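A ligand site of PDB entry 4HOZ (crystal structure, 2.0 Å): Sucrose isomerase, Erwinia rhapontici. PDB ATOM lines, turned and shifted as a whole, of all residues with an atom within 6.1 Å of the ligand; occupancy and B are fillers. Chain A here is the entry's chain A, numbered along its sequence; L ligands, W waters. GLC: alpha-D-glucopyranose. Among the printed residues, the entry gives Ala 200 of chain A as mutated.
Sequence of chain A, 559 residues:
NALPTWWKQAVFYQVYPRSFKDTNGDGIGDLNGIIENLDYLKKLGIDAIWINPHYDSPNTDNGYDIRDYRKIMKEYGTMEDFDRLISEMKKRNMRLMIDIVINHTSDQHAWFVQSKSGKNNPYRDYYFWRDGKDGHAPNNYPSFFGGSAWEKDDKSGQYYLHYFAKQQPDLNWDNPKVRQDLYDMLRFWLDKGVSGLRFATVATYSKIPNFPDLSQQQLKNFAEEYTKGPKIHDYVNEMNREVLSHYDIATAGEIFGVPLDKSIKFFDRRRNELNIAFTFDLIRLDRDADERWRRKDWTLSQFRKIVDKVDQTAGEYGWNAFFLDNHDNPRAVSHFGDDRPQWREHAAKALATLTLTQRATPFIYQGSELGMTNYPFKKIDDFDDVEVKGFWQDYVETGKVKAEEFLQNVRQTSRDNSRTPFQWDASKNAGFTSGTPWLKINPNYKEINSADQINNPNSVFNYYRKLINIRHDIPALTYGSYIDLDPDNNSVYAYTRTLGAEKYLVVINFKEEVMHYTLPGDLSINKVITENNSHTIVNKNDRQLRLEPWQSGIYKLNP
Water W1 lies within hydrogen-bond range of OD1 of Asp 61, O3 of the ligand, NH2 of Arg 419 and NH1 of Arg 415.
The side-chain carboxylate of Asp 61 is in salt-bridge range of the guanidinium group of Arg 415, 3.0 Å away.
The side-chain amide nitrogen of Gln 168 sits at hydrogen-bond distance from the side-chain carboxylate of Asp 61.
The guanidinium group (NH2) of Arg 419 lies within salt-bridge range of the side-chain carboxylate (OD1) of Asp 328 (3.2 Å).
OD1 of Asp 99 lies within salt-bridge range of NH1 of Arg 198 (2.9 Å).
A ring nitrogen (NE2) of His 104 lies within hydrogen-bond range of the backbone carbonyl oxygen (O) of Tyr 64.
The backbone carbonyl oxygen of Tyr 64 sits at hydrogen-bond distance from the side-chain amide nitrogen of Gln 168, at 3.0 Å.
The side-chain hydroxyl of Tyr 64 is in hydrogen-bond range of the side-chain carboxylate of Asp 99, at 2.6 Å.
A ring nitrogen (NE2) of His 104 sits at hydrogen-bond distance from the side-chain amide nitrogen of Gln 168 (3.5 Å).
Residues that only touch the ligand: Tyr 64, Phe 145, Phe 164, Ala 200, Thr 201 and Arg 419.
Within 4 Å of the ligand: Asp 61, Tyr 64, His 104, Phe 145, Phe 164, Gln 168, Arg 198, Ala 200, Thr 201, Glu 254, His 327, Asp 328, Arg 415 and Arg 419.
Along chain A the residues within 4 Å of the ligand span positions 61 to 419.
O1 of the ligand lies within hydrogen-bond range of OE1 of Glu 254, 2.4 Å away.
The side-chain carboxylate (OD2) of Asp 61 lies within hydrogen-bond range of an oxygen (O4) of the ligand, at 2.6 Å.
OD2 of Asp 328 is in hydrogen-bond range of O2 of the ligand, at 2.7 Å.
O4 of the ligand lies within hydrogen-bond range of NH2 of Arg 415 (2.8 Å).
A ring nitrogen (NE2) of His 327 is in hydrogen-bond range of an oxygen (O2) of the ligand (2.9 Å).
NH1 of Arg 198 is in hydrogen-bond range of O1 of the ligand, at 3.0 Å.
A ring nitrogen (NE2) of His 104 is in hydrogen-bond range of an oxygen (O6) of the ligand, 3.3 Å away.
NE2 of Gln 168 sits at hydrogen-bond distance from O6 of the ligand (3.3 Å).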
ATOM      1  N   TRP A  50     -37.385   2.382   1.876  1.00  0.00           N
ATOM      2  CA  TRP A  50     -36.394   3.383   2.302  1.00  0.00           C
ATOM      3  C   TRP A  50     -36.642   4.648   1.505  1.00  0.00           C
ATOM      4  O   TRP A  50     -36.664   4.602   0.269  1.00  0.00           O
ATOM      5  CB  TRP A  50     -34.939   2.842   2.163  1.00  0.00           C
ATOM      6  CG  TRP A  50     -33.889   3.991   2.041  1.00  0.00           C
ATOM      7  CD1 TRP A  50     -33.829   5.183   2.776  1.00  0.00           C
ATOM      8  CD2 TRP A  50     -32.775   4.052   1.116  1.00  0.00           C
ATOM      9  NE1 TRP A  50     -32.774   5.983   2.329  1.00  0.00           N
ATOM     10  CE2 TRP A  50     -32.111   5.357   1.338  1.00  0.00           C
ATOM     11  CE3 TRP A  50     -32.270   3.196   0.131  1.00  0.00           C
ATOM     12  CZ2 TRP A  50     -31.000   5.747   0.598  1.00  0.00           C
ATOM     13  CZ3 TRP A  50     -31.163   3.596  -0.607  1.00  0.00           C
ATOM     14  CH2 TRP A  50     -30.530   4.844  -0.384  1.00  0.00           C
ATOM     15  N   ASN A  52     -35.472   8.639   0.678  1.00  0.00           N
ATOM     16  CA  ASN A  52     -34.354   9.579   0.658  1.00  0.00           C
ATOM     17  C   ASN A  52     -34.787  10.739   1.563  1.00  0.00           C
ATOM     18  O   ASN A  52     -35.938  10.764   2.010  1.00  0.00           O
ATOM     19  CB  ASN A  52     -34.062  10.000  -0.772  1.00  0.00           C
ATOM     20  CG  ASN A  52     -33.483   8.848  -1.562  1.00  0.00           C
ATOM     21  OD1 ASN A  52     -34.200   8.139  -2.286  1.00  0.00           O
ATOM     22  ND2 ASN A  52     -32.156   8.617  -1.381  1.00  0.00           N
ATOM     23  N   ASP A  61     -28.525  19.862  -2.464  1.00  0.00           N
ATOM     24  CA  ASP A  61     -28.268  18.448  -2.798  1.00  0.00           C
ATOM     25  C   ASP A  61     -29.542  17.644  -2.533  1.00  0.00           C
ATOM     26  O   ASP A  61     -29.487  16.528  -1.993  1.00  0.00           O
ATOM     27  CB  ASP A  61     -27.065  17.931  -1.981  1.00  0.00           C
ATOM     28  CG  ASP A  61     -26.551  16.562  -2.478  1.00  0.00           C
ATOM     29  OD1 ASP A  61     -26.775  16.137  -3.639  1.00  0.00           O
ATOM     30  OD2 ASP A  61     -25.962  15.899  -1.639  1.00  0.00           O
ATOM     31  N   TYR A  64     -30.177  16.311   0.934  1.00  0.00           N
ATOM     32  CA  TYR A  64     -29.015  15.916   1.703  1.00  0.00           C
ATOM     33  C   TYR A  64     -28.323  17.109   2.407  1.00  0.00           C
ATOM     34  O   TYR A  64     -27.259  16.914   3.044  1.00  0.00           O
ATOM     35  CB  TYR A  64     -28.018  15.132   0.839  1.00  0.00           C
ATOM     36  CG  TYR A  64     -28.495  13.724   0.640  1.00  0.00           C
ATOM     37  CD1 TYR A  64     -29.281  13.380  -0.483  1.00  0.00           C
ATOM     38  CD2 TYR A  64     -28.296  12.746   1.630  1.00  0.00           C
ATOM     39  CE1 TYR A  64     -29.762  12.089  -0.669  1.00  0.00           C
ATOM     40  CE2 TYR A  64     -28.792  11.424   1.460  1.00  0.00           C
ATOM     41  CZ  TYR A  64     -29.521  11.131   0.304  1.00  0.00           C
ATOM     42  OH  TYR A  64     -30.037   9.878   0.132  1.00  0.00           O
ATOM     43  N   ASP A  65     -28.888  18.325   2.248  1.00  0.00           N
ATOM     44  CA  ASP A  65     -28.379  19.545   2.937  1.00  0.00           C
ATOM     45  C   ASP A  65     -29.523  19.992   3.889  1.00  0.00           C
ATOM     46  O   ASP A  65     -30.487  20.637   3.484  1.00  0.00           O
ATOM     47  CB  ASP A  65     -27.902  20.594   1.933  1.00  0.00           C
ATOM     48  CG  ASP A  65     -28.942  20.971   0.912  1.00  0.00           C
ATOM     49  OD1 ASP A  65     -29.580  20.067   0.307  1.00  0.00           O
ATOM     50  OD2 ASP A  65     -29.073  22.183   0.659  1.00  0.00           O
ATOM     51  N   ASP A  99     -33.519   8.208   5.946  1.00  0.00           N
ATOM     52  CA  ASP A  99     -32.170   8.502   5.585  1.00  0.00           C
ATOM     53  C   ASP A  99     -31.638   9.452   6.640  1.00  0.00           C
ATOM     54  O   ASP A  99     -32.198  10.537   6.821  1.00  0.00           O
ATOM     55  CB  ASP A  99     -32.197   9.238   4.227  1.00  0.00           C
ATOM     56  CG  ASP A  99     -30.952   9.008   3.410  1.00  0.00           C
ATOM     57  OD1 ASP A  99     -29.805   9.023   3.973  1.00  0.00           O
ATOM     58  OD2 ASP A  99     -31.113   8.795   2.184  1.00  0.00           O
ATOM     59  N   VAL A 101     -28.687  11.797   7.751  1.00  0.00           N
ATOM     60  CA  VAL A 101     -27.615  12.552   7.082  1.00  0.00           C
ATOM     61  C   VAL A 101     -26.937  13.406   8.154  1.00  0.00           C
ATOM     62  O   VAL A 101     -27.378  14.563   8.397  1.00  0.00           O
ATOM     63  CB  VAL A 101     -28.192  13.452   5.895  1.00  0.00           C
ATOM     64  CG1 VAL A 101     -27.055  14.117   5.072  1.00  0.00           C
ATOM     65  CG2 VAL A 101     -29.190  12.696   5.023  1.00  0.00           C
ATOM     66  N   HIS A 104     -22.902  16.091   7.966  1.00  0.00           N
ATOM     67  CA  HIS A 104     -22.922  17.548   7.694  1.00  0.00           C
ATOM     68  C   HIS A 104     -24.376  18.053   7.789  1.00  0.00           C
ATOM     69  O   HIS A 104     -25.329  17.253   7.832  1.00  0.00           O
ATOM     70  CB  HIS A 104     -22.313  17.785   6.311  1.00  0.00           C
ATOM     71  CG  HIS A 104     -22.961  16.924   5.216  1.00  0.00           C
ATOM     72  ND1 HIS A 104     -22.402  15.786   4.756  1.00  0.00           N
ATOM     73  CD2 HIS A 104     -24.172  17.068   4.529  1.00  0.00           C
ATOM     74  CE1 HIS A 104     -23.218  15.200   3.836  1.00  0.00           C
ATOM     75  NE2 HIS A 104     -24.301  15.971   3.703  1.00  0.00           N
ATOM     76  N   PHE A 145     -17.797  17.715  -4.422  1.00  0.00           N
ATOM     77  CA  PHE A 145     -18.739  18.435  -5.285  1.00  0.00           C
ATOM     78  C   PHE A 145     -18.087  19.663  -5.949  1.00  0.00           C
ATOM     79  O   PHE A 145     -18.803  20.523  -6.449  1.00  0.00           O
ATOM     80  CB  PHE A 145     -19.979  18.857  -4.490  1.00  0.00           C
ATOM     81  CG  PHE A 145     -20.936  17.716  -4.179  1.00  0.00           C
ATOM     82  CD1 PHE A 145     -20.742  16.427  -4.767  1.00  0.00           C
ATOM     83  CD2 PHE A 145     -22.021  17.939  -3.317  1.00  0.00           C
ATOM     84  CE1 PHE A 145     -21.643  15.390  -4.488  1.00  0.00           C
ATOM     85  CE2 PHE A 145     -22.933  16.920  -3.044  1.00  0.00           C
ATOM     86  CZ  PHE A 145     -22.745  15.654  -3.650  1.00  0.00           C
ATOM     87  N   PHE A 164     -18.594  17.829   1.005  1.00  0.00           N
ATOM     88  CA  PHE A 164     -19.588  17.904  -0.056  1.00  0.00           C
ATOM     89  C   PHE A 164     -19.753  19.357  -0.466  1.00  0.00           C
ATOM     90  O   PHE A 164     -18.713  20.013  -0.673  1.00  0.00           O
ATOM     91  CB  PHE A 164     -20.870  17.124   0.372  1.00  0.00           C
ATOM     92  CG  PHE A 164     -20.577  15.660   0.496  1.00  0.00           C
ATOM     93  CD1 PHE A 164     -20.182  15.106   1.723  1.00  0.00           C
ATOM     94  CD2 PHE A 164     -20.552  14.884  -0.634  1.00  0.00           C
ATOM     95  CE1 PHE A 164     -19.811  13.768   1.807  1.00  0.00           C
ATOM     96  CE2 PHE A 164     -20.180  13.551  -0.572  1.00  0.00           C
ATOM     97  CZ  PHE A 164     -19.868  12.973   0.655  1.00  0.00           C
ATOM     98  N   GLN A 168     -22.864  22.381   2.519  1.00  0.00           N
ATOM     99  CA  GLN A 168     -22.882  21.238   3.442  1.00  0.00           C
ATOM    100  C   GLN A 168     -21.698  21.198   4.430  1.00  0.00           C
ATOM    101  O   GLN A 168     -20.816  20.331   4.319  1.00  0.00           O
ATOM    102  CB  GLN A 168     -22.996  19.948   2.631  1.00  0.00           C
ATOM    103  CG  GLN A 168     -24.338  19.811   1.928  1.00  0.00           C
ATOM    104  CD  GLN A 168     -24.370  18.782   0.797  1.00  0.00           C
ATOM    105  OE1 GLN A 168     -23.629  18.873  -0.177  1.00  0.00           O
ATOM    106  NE2 GLN A 168     -25.281  17.810   0.919  1.00  0.00           N
ATOM    107  N   ARG A 198     -30.966   4.445   7.324  1.00  0.00           N
ATOM    108  CA  ARG A 198     -29.873   4.404   6.374  1.00  0.00           C
ATOM    109  C   ARG A 198     -28.930   5.598   6.637  1.00  0.00           C
ATOM    110  O   ARG A 198     -29.377   6.764   6.539  1.00  0.00           O
ATOM    111  CB  ARG A 198     -30.471   4.446   4.965  1.00  0.00           C
ATOM    112  CG  ARG A 198     -29.362   4.344   3.890  1.00  0.00           C
ATOM    113  CD  ARG A 198     -28.977   5.757   3.428  1.00  0.00           C
ATOM    114  NE  ARG A 198     -28.247   5.730   2.157  1.00  0.00           N
ATOM    115  CZ  ARG A 198     -27.698   6.802   1.586  1.00  0.00           C
ATOM    116  NH1 ARG A 198     -27.799   8.014   2.137  1.00  0.00           N
ATOM    117  NH2 ARG A 198     -27.061   6.641   0.426  1.00  0.00           N
ATOM    118  N   PHE A 199     -27.659   5.308   6.968  1.00  0.00           N
ATOM    119  CA  PHE A 199     -26.671   6.301   7.374  1.00  0.00           C
ATOM    120  C   PHE A 199     -25.870   6.718   6.164  1.00  0.00           C
ATOM    121  O   PHE A 199     -25.110   5.927   5.618  1.00  0.00           O
ATOM    122  CB  PHE A 199     -25.754   5.778   8.506  1.00  0.00           C
ATOM    123  CG  PHE A 199     -26.447   5.721   9.858  1.00  0.00           C
ATOM    124  CD1 PHE A 199     -27.085   4.538  10.280  1.00  0.00           C
ATOM    125  CD2 PHE A 199     -26.525   6.863  10.689  1.00  0.00           C
ATOM    126  CE1 PHE A 199     -27.759   4.496  11.518  1.00  0.00           C
ATOM    127  CE2 PHE A 199     -27.214   6.821  11.890  1.00  0.00           C
ATOM    128  CZ  PHE A 199     -27.816   5.628  12.330  1.00  0.00           C
ATOM    129  N   ALA A 200     -26.102   7.960   5.747  1.00  0.00           N
ATOM    130  CA  ALA A 200     -25.470   8.583   4.594  1.00  0.00           C
ATOM    131  C   ALA A 200     -24.025   8.817   4.893  1.00  0.00           C
ATOM    132  O   ALA A 200     -23.706   9.285   5.962  1.00  0.00           O
ATOM    133  CB  ALA A 200     -26.142   9.909   4.230  1.00  0.00           C
ATOM    134  N   THR A 201     -23.170   8.425   3.957  1.00  0.00           N
ATOM    135  CA  THR A 201     -21.720   8.505   4.081  1.00  0.00           C
ATOM    136  C   THR A 201     -21.252   8.339   5.519  1.00  0.00           C
ATOM    137  O   THR A 201     -20.589   9.233   6.114  1.00  0.00           O
ATOM    138  CB  THR A 201     -21.168   9.800   3.360  1.00  0.00           C
ATOM    139  OG1 THR A 201     -19.781   9.871   3.584  1.00  0.00           O
ATOM    140  CG2 THR A 201     -21.737  11.034   3.943  1.00  0.00           C
ATOM    141  N   GLU A 254     -23.942   3.383   4.591  1.00  0.00           N
ATOM    142  CA  GLU A 254     -23.417   3.709   3.252  1.00  0.00           C
ATOM    143  C   GLU A 254     -21.972   4.008   3.358  1.00  0.00           C
ATOM    144  O   GLU A 254     -21.605   5.141   3.694  1.00  0.00           O
ATOM    145  CB  GLU A 254     -24.160   4.878   2.604  1.00  0.00           C
ATOM    146  CG  GLU A 254     -23.642   5.140   1.170  1.00  0.00           C
ATOM    147  CD  GLU A 254     -23.816   6.589   0.700  1.00  0.00           C
ATOM    148  OE1 GLU A 254     -23.850   7.523   1.513  1.00  0.00           O
ATOM    149  OE2 GLU A 254     -23.904   6.779  -0.541  1.00  0.00           O
ATOM    150  N   HIS A 327     -30.374   6.249  -6.465  1.00  0.00           N
ATOM    151  CA  HIS A 327     -30.560   7.654  -6.898  1.00  0.00           C
ATOM    152  C   HIS A 327     -29.165   8.265  -7.147  1.00  0.00           C
ATOM    153  O   HIS A 327     -29.049   9.464  -7.506  1.00  0.00           O
ATOM    154  CB  HIS A 327     -31.267   8.458  -5.772  1.00  0.00           C
ATOM    155  CG  HIS A 327     -30.430   8.510  -4.477  1.00  0.00           C
ATOM    156  ND1 HIS A 327     -30.055   7.372  -3.803  1.00  0.00           N
ATOM    157  CD2 HIS A 327     -29.803   9.585  -3.812  1.00  0.00           C
ATOM    158  CE1 HIS A 327     -29.273   7.715  -2.753  1.00  0.00           C
ATOM    159  NE2 HIS A 327     -29.123   9.078  -2.760  1.00  0.00           N
ATOM    160  N   ASP A 328     -28.088   7.514  -6.883  1.00  0.00           N
ATOM    161  CA  ASP A 328     -26.728   8.046  -7.139  1.00  0.00           C
ATOM    162  C   ASP A 328     -26.024   7.433  -8.371  1.00  0.00           C
ATOM    163  O   ASP A 328     -24.820   7.673  -8.569  1.00  0.00           O
ATOM    164  CB  ASP A 328     -25.824   7.838  -5.958  1.00  0.00           C
ATOM    165  CG  ASP A 328     -26.151   8.728  -4.806  1.00  0.00           C
ATOM    166  OD1 ASP A 328     -26.744   9.828  -4.998  1.00  0.00           O
ATOM    167  OD2 ASP A 328     -25.783   8.326  -3.643  1.00  0.00           O
ATOM    168  N   ARG A 415     -25.817  10.850 -11.885  1.00  0.00           N
ATOM    169  CA  ARG A 415     -26.868  10.523 -10.910  1.00  0.00           C
ATOM    170  C   ARG A 415     -28.297  10.898 -11.426  1.00  0.00           C
ATOM    171  O   ARG A 415     -29.303  10.283 -11.050  1.00  0.00           O
ATOM    172  CB  ARG A 415     -26.547  11.200  -9.583  1.00  0.00           C
ATOM    173  CG  ARG A 415     -25.116  11.034  -9.141  1.00  0.00           C
ATOM    174  CD  ARG A 415     -24.866  11.359  -7.638  1.00  0.00           C
ATOM    175  NE  ARG A 415     -25.160  12.787  -7.290  1.00  0.00           N
ATOM    176  CZ  ARG A 415     -25.106  13.261  -6.053  1.00  0.00           C
ATOM    177  NH1 ARG A 415     -25.373  14.571  -5.780  1.00  0.00           N
ATOM    178  NH2 ARG A 415     -24.775  12.411  -5.049  1.00  0.00           N
ATOM    179  N   ARG A 419     -32.974   9.954 -11.590  1.00  0.00           N
ATOM    180  CA  ARG A 419     -33.859  10.944 -10.972  1.00  0.00           C
ATOM    181  C   ARG A 419     -34.971  11.460 -11.889  1.00  0.00           C
ATOM    182  O   ARG A 419     -35.777  12.234 -11.421  1.00  0.00           O
ATOM    183  CB  ARG A 419     -33.065  12.109 -10.372  1.00  0.00           C
ATOM    184  CG  ARG A 419     -31.987  11.586  -9.431  1.00  0.00           C
ATOM    185  CD  ARG A 419     -31.058  12.676  -8.905  1.00  0.00           C
ATOM    186  NE  ARG A 419     -30.082  12.068  -7.969  1.00  0.00           N
ATOM    187  CZ  ARG A 419     -29.371  12.797  -7.114  1.00  0.00           C
ATOM    188  NH1 ARG A 419     -29.511  14.142  -7.137  1.00  0.00           N
ATOM    189  NH2 ARG A 419     -28.499  12.220  -6.287  1.00  0.00           N
HETATM  190  C1  GLC L   1     -25.557  10.591   0.478  1.00  0.00           C
HETATM  191  C2  GLC L   1     -26.363  10.412  -0.830  1.00  0.00           C
HETATM  192  C3  GLC L   1     -25.943  11.300  -1.996  1.00  0.00           C
HETATM  193  C4  GLC L   1     -25.520  12.675  -1.465  1.00  0.00           C
HETATM  194  C5  GLC L   1     -24.338  12.505  -0.488  1.00  0.00           C
HETATM  195  C6  GLC L   1     -23.900  13.791   0.219  1.00  0.00           C
HETATM  196  O1  GLC L   1     -25.364   9.427   1.254  1.00  0.00           O
HETATM  197  O2  GLC L   1     -26.608   9.111  -1.237  1.00  0.00           O
HETATM  198  O3  GLC L   1     -27.024  11.395  -2.863  1.00  0.00           O
HETATM  199  O4  GLC L   1     -25.189  13.541  -2.522  1.00  0.00           O
HETATM  200  O5  GLC L   1     -24.480  11.498   0.494  1.00  0.00           O
HETATM  201  O6  GLC L   1     -24.943  14.515   0.800  1.00  0.00           O
HETATM  202  O   HOH W   1     -28.101  13.825  -3.835  1.00  0.00           O
